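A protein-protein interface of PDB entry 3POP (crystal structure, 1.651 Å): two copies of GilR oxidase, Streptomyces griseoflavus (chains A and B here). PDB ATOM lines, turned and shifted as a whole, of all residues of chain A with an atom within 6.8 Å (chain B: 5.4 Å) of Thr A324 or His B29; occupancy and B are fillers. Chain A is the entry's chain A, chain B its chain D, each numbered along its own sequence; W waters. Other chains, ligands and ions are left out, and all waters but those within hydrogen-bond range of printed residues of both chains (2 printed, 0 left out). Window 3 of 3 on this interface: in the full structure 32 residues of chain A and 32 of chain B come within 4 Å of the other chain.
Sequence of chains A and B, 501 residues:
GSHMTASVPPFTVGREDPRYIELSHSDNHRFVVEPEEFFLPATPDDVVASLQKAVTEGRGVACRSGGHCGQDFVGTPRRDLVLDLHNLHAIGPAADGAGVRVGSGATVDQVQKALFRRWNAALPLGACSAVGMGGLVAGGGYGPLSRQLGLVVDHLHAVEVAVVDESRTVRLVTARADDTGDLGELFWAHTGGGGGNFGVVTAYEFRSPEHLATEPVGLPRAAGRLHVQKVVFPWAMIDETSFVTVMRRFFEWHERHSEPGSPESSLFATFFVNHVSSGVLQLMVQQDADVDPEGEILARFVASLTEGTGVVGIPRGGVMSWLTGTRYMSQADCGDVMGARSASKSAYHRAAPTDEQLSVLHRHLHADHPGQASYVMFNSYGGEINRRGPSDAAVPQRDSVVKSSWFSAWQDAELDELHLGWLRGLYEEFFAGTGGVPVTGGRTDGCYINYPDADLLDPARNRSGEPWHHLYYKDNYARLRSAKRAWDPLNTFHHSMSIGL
Water W1 bridges OG1 of Thr A324 and O of Ser B26. Water W2 lies within hydrogen-bond range of the side-chain carboxylate (OE1) of Glu B22 (2.8 Å) and the guanidinium group (NH1) of Arg A327 (3.4 Å).
Printed residues of chain A that touch a printed residue of chain B: Ser A321, Trp A322, Leu A323, Thr A324, Arg A327 and Tyr A328. Of the 13 printed residues of chain B, 5 touch a printed residue of chain A. Printed residues of chain B that touch a printed residue of chain A: Glu B22, His B25, His B29, Met B338 and Gly B339. Hydrophobic or aromatic side chains of chain B within 4 Å of the printed part of chain A: His B25, His B29 and Met B338. Among the printed residues, 10 pairs touch across the chains. Among the printed residues, Asp or Glu carboxylates within 4 Å of a Lys or Arg side-chain nitrogen of the other chain: Arg A327 with Glu B22.
Of chain B, only Glu B22, His B29 and Gly B339 come within 4 Å of Thr A324. Printed residues of chain B within 4 Å of Arg A327: Glu B22 (3.5 Å) and Met B338 (3.6 Å). Of the printed residues of chain B, Tyr A328 touches Met B338 (3.5 Å). Of the printed residues of chain A, Glu B22 touches Ser A321 (2.7 Å), Trp A322 (3.8 Å), Leu A323 (3.1 Å), Thr A324 (2.6 Å) and Arg A327 (3.5 Å). Of the printed residues of chain A, His B25 touches Ser A321 (3.8 Å). Of chain A, only Thr A324 (3.9 Å) comes within 4 Å of His B29. Phe B31 touches none of the printed residues of chain A. Ser B342 touches none of the printed residues of chain A. The nearest residue of chain B that does not touch Thr A324 is Met B338 (4.3 Å).
No position is printed for both chains.
The backbone carbonyl oxygen (O) of Trp A322 is in hydrogen-bond range of the side-chain hydroxyl (OG1) of Thr A326 (2.8 Å). O of Leu A323 lies within hydrogen-bond range of NE of Arg A327 (3.1 Å). The backbone carbonyl oxygen (O) of Ser B26 lies within hydrogen-bond range of a ring nitrogen (ND1) of His B29 (3.3 Å). ND1 of His B29 is in hydrogen-bond range of O of Asp B27 (3.2 Å). N of His B29 lies within hydrogen-bond range of O of Ala B340, 2.9 Å away. The backbone carbonyl oxygen of His B29 lies within hydrogen-bond range of the guanidinium group of Arg B341, at 3.2 Å.
CD2 of His B25 touches OG of Ser A321 (3.8 Å). Trp A322 touches Glu B22. CG2 of Thr A324 touches NE2 of His B29 (3.9 Å). N of Gly B339 touches CG2 of Thr A324 (3.8 Å). Arg A327 touches Met B338. Met B338 touches Tyr A328 (O to CD1, 3.5 Å).
OE2 of Glu B22 is in hydrogen-bond range of OG of Ser A321 (2.7 Å). The backbone NH of Leu A323 is in hydrogen-bond range of the side-chain carboxylate of Glu B22 (3.1 Å). The side-chain hydroxyl (OG1) of Thr A324 sits at hydrogen-bond distance from the side-chain carboxylate (OE1) of Glu B22 (2.6 Å). The guanidinium group (NH1) of Arg A327 is in salt-bridge range of the side-chain carboxylate (OE1) of Glu B22 (3.5 Å).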
ATOM      1  N   LEU A 226     -11.981  -1.965 -18.800  1.00  0.00           N
ATOM      2  CA  LEU A 226     -11.844  -0.519 -18.788  1.00  0.00           C
ATOM      3  C   LEU A 226     -11.486  -0.024 -20.165  1.00  0.00           C
ATOM      4  O   LEU A 226     -10.559  -0.547 -20.790  1.00  0.00           O
ATOM      5  CB  LEU A 226     -10.707  -0.090 -17.845  1.00  0.00           C
ATOM      6  CG  LEU A 226     -10.818  -0.466 -16.378  1.00  0.00           C
ATOM      7  CD1 LEU A 226      -9.508  -0.112 -15.660  1.00  0.00           C
ATOM      8  CD2 LEU A 226     -11.991   0.271 -15.728  1.00  0.00           C
ATOM      9  N   VAL A 228      -9.376   2.599 -21.949  1.00  0.00           N
ATOM     10  CA  VAL A 228      -8.245   3.421 -21.532  1.00  0.00           C
ATOM     11  C   VAL A 228      -7.722   4.124 -22.762  1.00  0.00           C
ATOM     12  O   VAL A 228      -7.541   3.510 -23.811  1.00  0.00           O
ATOM     13  CB  VAL A 228      -7.123   2.593 -20.873  1.00  0.00           C
ATOM     14  CG1 VAL A 228      -7.605   2.034 -19.544  1.00  0.00           C
ATOM     15  CG2 VAL A 228      -6.667   1.467 -21.798  1.00  0.00           C
ATOM     16  N   MET A 320      -9.163  -2.841 -21.902  1.00  0.00           N
ATOM     17  CA  MET A 320      -8.287  -3.760 -21.194  1.00  0.00           C
ATOM     18  C   MET A 320      -9.003  -4.347 -19.993  1.00  0.00           C
ATOM     19  O   MET A 320     -10.007  -3.806 -19.519  1.00  0.00           O
ATOM     20  CB  MET A 320      -7.030  -3.020 -20.715  1.00  0.00           C
ATOM     21  CG  MET A 320      -6.175  -2.457 -21.851  1.00  0.00           C
ATOM     22  SD  MET A 320      -4.571  -1.858 -21.279  1.00  0.00           S
ATOM     23  CE  MET A 320      -3.968  -1.091 -22.797  1.00  0.00           C
ATOM     24  N   SER A 321      -8.491  -5.465 -19.497  1.00  0.00           N
ATOM     25  CA  SER A 321      -9.018  -6.032 -18.278  1.00  0.00           C
ATOM     26  C   SER A 321      -8.587  -5.119 -17.133  1.00  0.00           C
ATOM     27  O   SER A 321      -7.765  -4.229 -17.325  1.00  0.00           O
ATOM     28  CB  SER A 321      -8.524  -7.473 -18.088  1.00  0.00           C
ATOM     29  OG  SER A 321      -7.140  -7.579 -18.355  1.00  0.00           O
ATOM     30  N   TRP A 322      -9.140  -5.336 -15.947  1.00  0.00           N
ATOM     31  CA  TRP A 322      -9.027  -4.342 -14.877  1.00  0.00           C
ATOM     32  C   TRP A 322      -7.607  -4.094 -14.394  1.00  0.00           C
ATOM     33  O   TRP A 322      -7.165  -2.939 -14.301  1.00  0.00           O
ATOM     34  CB  TRP A 322      -9.894  -4.708 -13.680  1.00  0.00           C
ATOM     35  CG  TRP A 322      -9.998  -3.541 -12.709  1.00  0.00           C
ATOM     36  CD1 TRP A 322     -10.926  -2.535 -12.733  1.00  0.00           C
ATOM     37  CD2 TRP A 322      -9.129  -3.260 -11.612  1.00  0.00           C
ATOM     38  NE1 TRP A 322     -10.684  -1.646 -11.707  1.00  0.00           N
ATOM     39  CE2 TRP A 322      -9.590  -2.077 -11.001  1.00  0.00           C
ATOM     40  CE3 TRP A 322      -8.005  -3.901 -11.082  1.00  0.00           C
ATOM     41  CZ2 TRP A 322      -8.945  -1.501  -9.897  1.00  0.00           C
ATOM     42  CZ3 TRP A 322      -7.374  -3.345  -9.989  1.00  0.00           C
ATOM     43  CH2 TRP A 322      -7.852  -2.159  -9.396  1.00  0.00           C
ATOM     44  N   LEU A 323      -6.884  -5.161 -14.081  1.00  0.00           N
ATOM     45  CA  LEU A 323      -5.571  -4.994 -13.472  1.00  0.00           C
ATOM     46  C   LEU A 323      -4.554  -4.483 -14.493  1.00  0.00           C
ATOM     47  O   LEU A 323      -3.705  -3.638 -14.172  1.00  0.00           O
ATOM     48  CB  LEU A 323      -5.113  -6.295 -12.819  1.00  0.00           C
ATOM     49  CG  LEU A 323      -3.912  -6.221 -11.876  1.00  0.00           C
ATOM     50  CD1 LEU A 323      -4.231  -5.317 -10.684  1.00  0.00           C
ATOM     51  CD2 LEU A 323      -3.546  -7.617 -11.384  1.00  0.00           C
ATOM     52  N   THR A 324      -4.633  -4.991 -15.721  1.00  0.00           N
ATOM     53  CA  THR A 324      -3.762  -4.515 -16.791  1.00  0.00           C
ATOM     54  C   THR A 324      -4.055  -3.063 -17.179  1.00  0.00           C
ATOM     55  O   THR A 324      -3.131  -2.263 -17.372  1.00  0.00           O
ATOM     56  CB  THR A 324      -3.829  -5.470 -18.017  1.00  0.00           C
ATOM     57  OG1 THR A 324      -3.221  -6.713 -17.638  1.00  0.00           O
ATOM     58  CG2 THR A 324      -3.052  -4.893 -19.196  1.00  0.00           C
ATOM     59  N   GLY A 325      -5.333  -2.720 -17.260  1.00  0.00           N
ATOM     60  CA  GLY A 325      -5.738  -1.365 -17.603  1.00  0.00           C
ATOM     61  C   GLY A 325      -5.360  -0.366 -16.523  1.00  0.00           C
ATOM     62  O   GLY A 325      -4.885   0.715 -16.811  1.00  0.00           O
ATOM     63  N   THR A 326      -5.547  -0.751 -15.266  1.00  0.00           N
ATOM     64  CA  THR A 326      -5.164   0.110 -14.159  1.00  0.00           C
ATOM     65  C   THR A 326      -3.666   0.382 -14.203  1.00  0.00           C
ATOM     66  O   THR A 326      -3.235   1.531 -14.012  1.00  0.00           O
ATOM     67  CB  THR A 326      -5.575  -0.514 -12.836  1.00  0.00           C
ATOM     68  OG1 THR A 326      -7.003  -0.624 -12.821  1.00  0.00           O
ATOM     69  CG2 THR A 326      -5.116   0.352 -11.658  1.00  0.00           C
ATOM     70  N   ARG A 327      -2.857  -0.649 -14.464  1.00  0.00           N
ATOM     71  CA  ARG A 327      -1.415  -0.438 -14.515  1.00  0.00           C
ATOM     72  C   ARG A 327      -1.020   0.402 -15.716  1.00  0.00           C
ATOM     73  O   ARG A 327      -0.121   1.242 -15.639  1.00  0.00           O
ATOM     74  CB  ARG A 327      -0.668  -1.769 -14.486  1.00  0.00           C
ATOM     75  CG  ARG A 327      -0.701  -2.357 -13.071  1.00  0.00           C
ATOM     76  CD  ARG A 327      -0.053  -3.731 -13.010  1.00  0.00           C
ATOM     77  NE  ARG A 327      -0.801  -4.689 -13.818  1.00  0.00           N
ATOM     78  CZ  ARG A 327      -0.403  -5.936 -14.057  1.00  0.00           C
ATOM     79  NH1 ARG A 327      -1.148  -6.750 -14.804  1.00  0.00           N
ATOM     80  NH2 ARG A 327       0.739  -6.372 -13.543  1.00  0.00           N
ATOM     81  N   TYR A 328      -1.703   0.203 -16.833  1.00  0.00           N
ATOM     82  CA  TYR A 328      -1.415   0.984 -18.028  1.00  0.00           C
ATOM     83  C   TYR A 328      -1.594   2.483 -17.757  1.00  0.00           C
ATOM     84  O   TYR A 328      -0.886   3.322 -18.320  1.00  0.00           O
ATOM     85  CB  TYR A 328      -2.369   0.548 -19.140  1.00  0.00           C
ATOM     86  CG  TYR A 328      -2.284   1.315 -20.439  1.00  0.00           C
ATOM     87  CD1 TYR A 328      -1.213   1.117 -21.315  1.00  0.00           C
ATOM     88  CD2 TYR A 328      -3.312   2.163 -20.846  1.00  0.00           C
ATOM     89  CE1 TYR A 328      -1.147   1.770 -22.525  1.00  0.00           C
ATOM     90  CE2 TYR A 328      -3.248   2.824 -22.083  1.00  0.00           C
ATOM     91  CZ  TYR A 328      -2.166   2.622 -22.908  1.00  0.00           C
ATOM     92  OH  TYR A 328      -2.104   3.265 -24.131  1.00  0.00           O
ATOM     93  N   MET A 329      -2.535   2.817 -16.884  1.00  0.00           N
ATOM     94  CA  MET A 329      -2.825   4.228 -16.592  1.00  0.00           C
ATOM     95  C   MET A 329      -2.056   4.763 -15.382  1.00  0.00           C
ATOM     96  O   MET A 329      -2.232   5.932 -15.008  1.00  0.00           O
ATOM     97  CB  MET A 329      -4.332   4.433 -16.339  1.00  0.00           C
ATOM     98  CG  MET A 329      -5.249   3.972 -17.488  1.00  0.00           C
ATOM     99  SD  MET A 329      -4.946   4.922 -18.994  1.00  0.00           S
ATOM    100  CE  MET A 329      -6.037   6.321 -18.685  1.00  0.00           C
ATOM    101  N   GLU B  22      -8.611 -11.169 -16.906  1.00  0.00           N
ATOM    102  CA  GLU B  22      -7.263 -10.705 -16.575  1.00  0.00           C
ATOM    103  C   GLU B  22      -6.246 -11.848 -16.642  1.00  0.00           C
ATOM    104  O   GLU B  22      -5.162 -11.700 -17.217  1.00  0.00           O
ATOM    105  CB  GLU B  22      -7.251 -10.010 -15.190  1.00  0.00           C
ATOM    106  CG  GLU B  22      -5.858  -9.591 -14.731  1.00  0.00           C
ATOM    107  CD  GLU B  22      -5.286  -8.445 -15.558  1.00  0.00           C
ATOM    108  OE1 GLU B  22      -4.060  -8.452 -15.836  1.00  0.00           O
ATOM    109  OE2 GLU B  22      -6.059  -7.523 -15.911  1.00  0.00           O
ATOM    110  N   HIS B  25      -4.461 -13.227 -19.956  1.00  0.00           N
ATOM    111  CA  HIS B  25      -3.399 -12.474 -20.611  1.00  0.00           C
ATOM    112  C   HIS B  25      -2.141 -12.619 -19.779  1.00  0.00           C
ATOM    113  O   HIS B  25      -2.189 -12.428 -18.562  1.00  0.00           O
ATOM    114  CB  HIS B  25      -3.733 -10.976 -20.632  1.00  0.00           C
ATOM    115  CG  HIS B  25      -4.966 -10.633 -21.407  1.00  0.00           C
ATOM    116  ND1 HIS B  25      -5.070 -10.836 -22.768  1.00  0.00           N
ATOM    117  CD2 HIS B  25      -6.142 -10.088 -21.013  1.00  0.00           C
ATOM    118  CE1 HIS B  25      -6.263 -10.437 -23.178  1.00  0.00           C
ATOM    119  NE2 HIS B  25      -6.932  -9.977 -22.132  1.00  0.00           N
ATOM    120  N   SER B  26      -1.021 -12.920 -20.427  1.00  0.00           N
ATOM    121  CA  SER B  26       0.287 -12.722 -19.808  1.00  0.00           C
ATOM    122  C   SER B  26       0.807 -11.353 -20.252  1.00  0.00           C
ATOM    123  O   SER B  26       0.069 -10.557 -20.828  1.00  0.00           O
ATOM    124  CB  SER B  26       1.252 -13.821 -20.248  1.00  0.00           C
ATOM    125  OG  SER B  26       0.768 -15.102 -19.860  1.00  0.00           O
ATOM    126  N   ASP B  27       2.073 -11.047 -19.991  1.00  0.00           N
ATOM    127  CA  ASP B  27       2.548  -9.732 -20.386  1.00  0.00           C
ATOM    128  C   ASP B  27       2.436  -9.439 -21.893  1.00  0.00           C
ATOM    129  O   ASP B  27       2.071  -8.328 -22.293  1.00  0.00           O
ATOM    130  CB  ASP B  27       3.973  -9.500 -19.922  1.00  0.00           C
ATOM    131  CG  ASP B  27       4.325  -8.010 -19.908  1.00  0.00           C
ATOM    132  OD1 ASP B  27       3.692  -7.230 -19.139  1.00  0.00           O
ATOM    133  OD2 ASP B  27       5.217  -7.625 -20.689  1.00  0.00           O
ATOM    134  N   ASN B  28       2.755 -10.431 -22.723  1.00  0.00           N
ATOM    135  CA  ASN B  28       2.737 -10.246 -24.175  1.00  0.00           C
ATOM    136  C   ASN B  28       1.331 -10.537 -24.684  1.00  0.00           C
ATOM    137  O   ASN B  28       0.883 -11.679 -24.665  1.00  0.00           O
ATOM    138  CB  ASN B  28       3.746 -11.205 -24.843  1.00  0.00           C
ATOM    139  CG  ASN B  28       4.000 -10.877 -26.301  1.00  0.00           C
ATOM    140  OD1 ASN B  28       5.048 -11.225 -26.863  1.00  0.00           O
ATOM    141  ND2 ASN B  28       3.047 -10.212 -26.926  1.00  0.00           N
ATOM    142  N   HIS B  29       0.628  -9.497 -25.113  1.00  0.00           N
ATOM    143  CA  HIS B  29      -0.769  -9.657 -25.511  1.00  0.00           C
ATOM    144  C   HIS B  29      -0.989 -10.282 -26.894  1.00  0.00           C
ATOM    145  O   HIS B  29      -2.130 -10.433 -27.339  1.00  0.00           O
ATOM    146  CB  HIS B  29      -1.516  -8.332 -25.368  1.00  0.00           C
ATOM    147  CG  HIS B  29      -1.929  -8.025 -23.960  1.00  0.00           C
ATOM    148  ND1 HIS B  29      -1.084  -8.175 -22.879  1.00  0.00           N
ATOM    149  CD2 HIS B  29      -3.105  -7.585 -23.455  1.00  0.00           C
ATOM    150  CE1 HIS B  29      -1.725  -7.844 -21.771  1.00  0.00           C
ATOM    151  NE2 HIS B  29      -2.951  -7.483 -22.094  1.00  0.00           N
ATOM    152  N   ARG B  30       0.092 -10.668 -27.571  1.00  0.00           N
ATOM    153  CA  ARG B  30      -0.036 -11.446 -28.812  1.00  0.00           C
ATOM    154  C   ARG B  30      -0.615 -12.819 -28.538  1.00  0.00           C
ATOM    155  O   ARG B  30      -1.158 -13.478 -29.433  1.00  0.00           O
ATOM    156  CB  ARG B  30       1.323 -11.629 -29.490  1.00  0.00           C
ATOM    157  CG  ARG B  30       1.802 -10.403 -30.187  1.00  0.00           C
ATOM    158  CD  ARG B  30       3.207 -10.583 -30.700  1.00  0.00           C
ATOM    159  NE  ARG B  30       3.263 -11.707 -31.601  1.00  0.00           N
ATOM    160  CZ  ARG B  30       4.317 -12.492 -31.781  1.00  0.00           C
ATOM    161  NH1 ARG B  30       5.447 -12.290 -31.125  1.00  0.00           N
ATOM    162  NH2 ARG B  30       4.225 -13.499 -32.631  1.00  0.00           N
ATOM    163  N   PHE B  31      -0.501 -13.267 -27.301  1.00  0.00           N
ATOM    164  CA  PHE B  31      -0.881 -14.624 -26.979  1.00  0.00           C
ATOM    165  C   PHE B  31      -1.953 -14.600 -25.911  1.00  0.00           C
ATOM    166  O   PHE B  31      -2.046 -13.661 -25.139  1.00  0.00           O
ATOM    167  CB  PHE B  31       0.353 -15.427 -26.531  1.00  0.00           C
ATOM    168  CG  PHE B  31       1.526 -15.291 -27.469  1.00  0.00           C
ATOM    169  CD1 PHE B  31       2.710 -14.719 -27.045  1.00  0.00           C
ATOM    170  CD2 PHE B  31       1.414 -15.685 -28.793  1.00  0.00           C
ATOM    171  CE1 PHE B  31       3.770 -14.556 -27.922  1.00  0.00           C
ATOM    172  CE2 PHE B  31       2.477 -15.541 -29.670  1.00  0.00           C
ATOM    173  CZ  PHE B  31       3.653 -14.973 -29.231  1.00  0.00           C
ATOM    174  N   MET B 338       2.580  -1.900 -20.760  1.00  0.00           N
ATOM    175  CA  MET B 338       1.464  -2.759 -20.337  1.00  0.00           C
ATOM    176  C   MET B 338       0.401  -2.956 -21.419  1.00  0.00           C
ATOM    177  O   MET B 338       0.024  -2.016 -22.133  1.00  0.00           O
ATOM    178  CB  MET B 338       0.793  -2.209 -19.069  1.00  0.00           C
ATOM    179  CG  MET B 338       1.744  -2.031 -17.893  1.00  0.00           C
ATOM    180  SD  MET B 338       2.534  -3.579 -17.384  1.00  0.00           S
ATOM    181  CE  MET B 338       1.099  -4.582 -16.977  1.00  0.00           C
ATOM    182  N   GLY B 339      -0.098  -4.181 -21.521  1.00  0.00           N
ATOM    183  CA  GLY B 339      -1.082  -4.523 -22.536  1.00  0.00           C
ATOM    184  C   GLY B 339      -0.610  -4.474 -23.989  1.00  0.00           C
ATOM    185  O   GLY B 339      -1.431  -4.401 -24.904  1.00  0.00           O
ATOM    186  N   ALA B 340       0.699  -4.509 -24.216  1.00  0.00           N
ATOM    187  CA  ALA B 340       1.218  -4.426 -25.572  1.00  0.00           C
ATOM    188  C   ALA B 340       1.473  -5.803 -26.195  1.00  0.00           C
ATOM    189  O   ALA B 340       1.685  -6.809 -25.512  1.00  0.00           O
ATOM    190  CB  ALA B 340       2.501  -3.530 -25.644  1.00  0.00           C
ATOM    191  N   ARG B 341       1.436  -5.820 -27.514  1.00  0.00           N
ATOM    192  CA  ARG B 341       1.842  -6.966 -28.296  1.00  0.00           C
ATOM    193  C   ARG B 341       3.317  -6.762 -28.612  1.00  0.00           C
ATOM    194  O   ARG B 341       3.740  -5.643 -28.893  1.00  0.00           O
ATOM    195  CB  ARG B 341       1.035  -7.005 -29.585  1.00  0.00           C
ATOM    196  CG  ARG B 341      -0.472  -7.021 -29.344  1.00  0.00           C
ATOM    197  CD  ARG B 341      -1.249  -6.977 -30.670  1.00  0.00           C
ATOM    198  NE  ARG B 341      -1.285  -8.262 -31.359  1.00  0.00           N
ATOM    199  CZ  ARG B 341      -2.154  -9.238 -31.092  1.00  0.00           C
ATOM    200  NH1 ARG B 341      -3.045  -9.080 -30.118  1.00  0.00           N
ATOM    201  NH2 ARG B 341      -2.137 -10.361 -31.802  1.00  0.00           N
ATOM    202  N   SER B 342       4.116  -7.812 -28.529  1.00  0.00           N
ATOM    203  CA  SER B 342       5.538  -7.605 -28.808  1.00  0.00           C
ATOM    204  C   SER B 342       6.225  -8.821 -29.400  1.00  0.00           C
ATOM    205  O   SER B 342       5.692  -9.933 -29.402  1.00  0.00           O
ATOM    206  CB  SER B 342       6.289  -7.119 -27.568  1.00  0.00           C
ATOM    207  OG  SER B 342       6.304  -8.117 -26.559  1.00  0.00           O
HETATM  208  O   HOH W   1      -1.171  -7.875 -19.015  1.00  0.00           O
HETATM  209  O   HOH W   2      -2.055 -10.025 -14.637  1.00  0.00           O
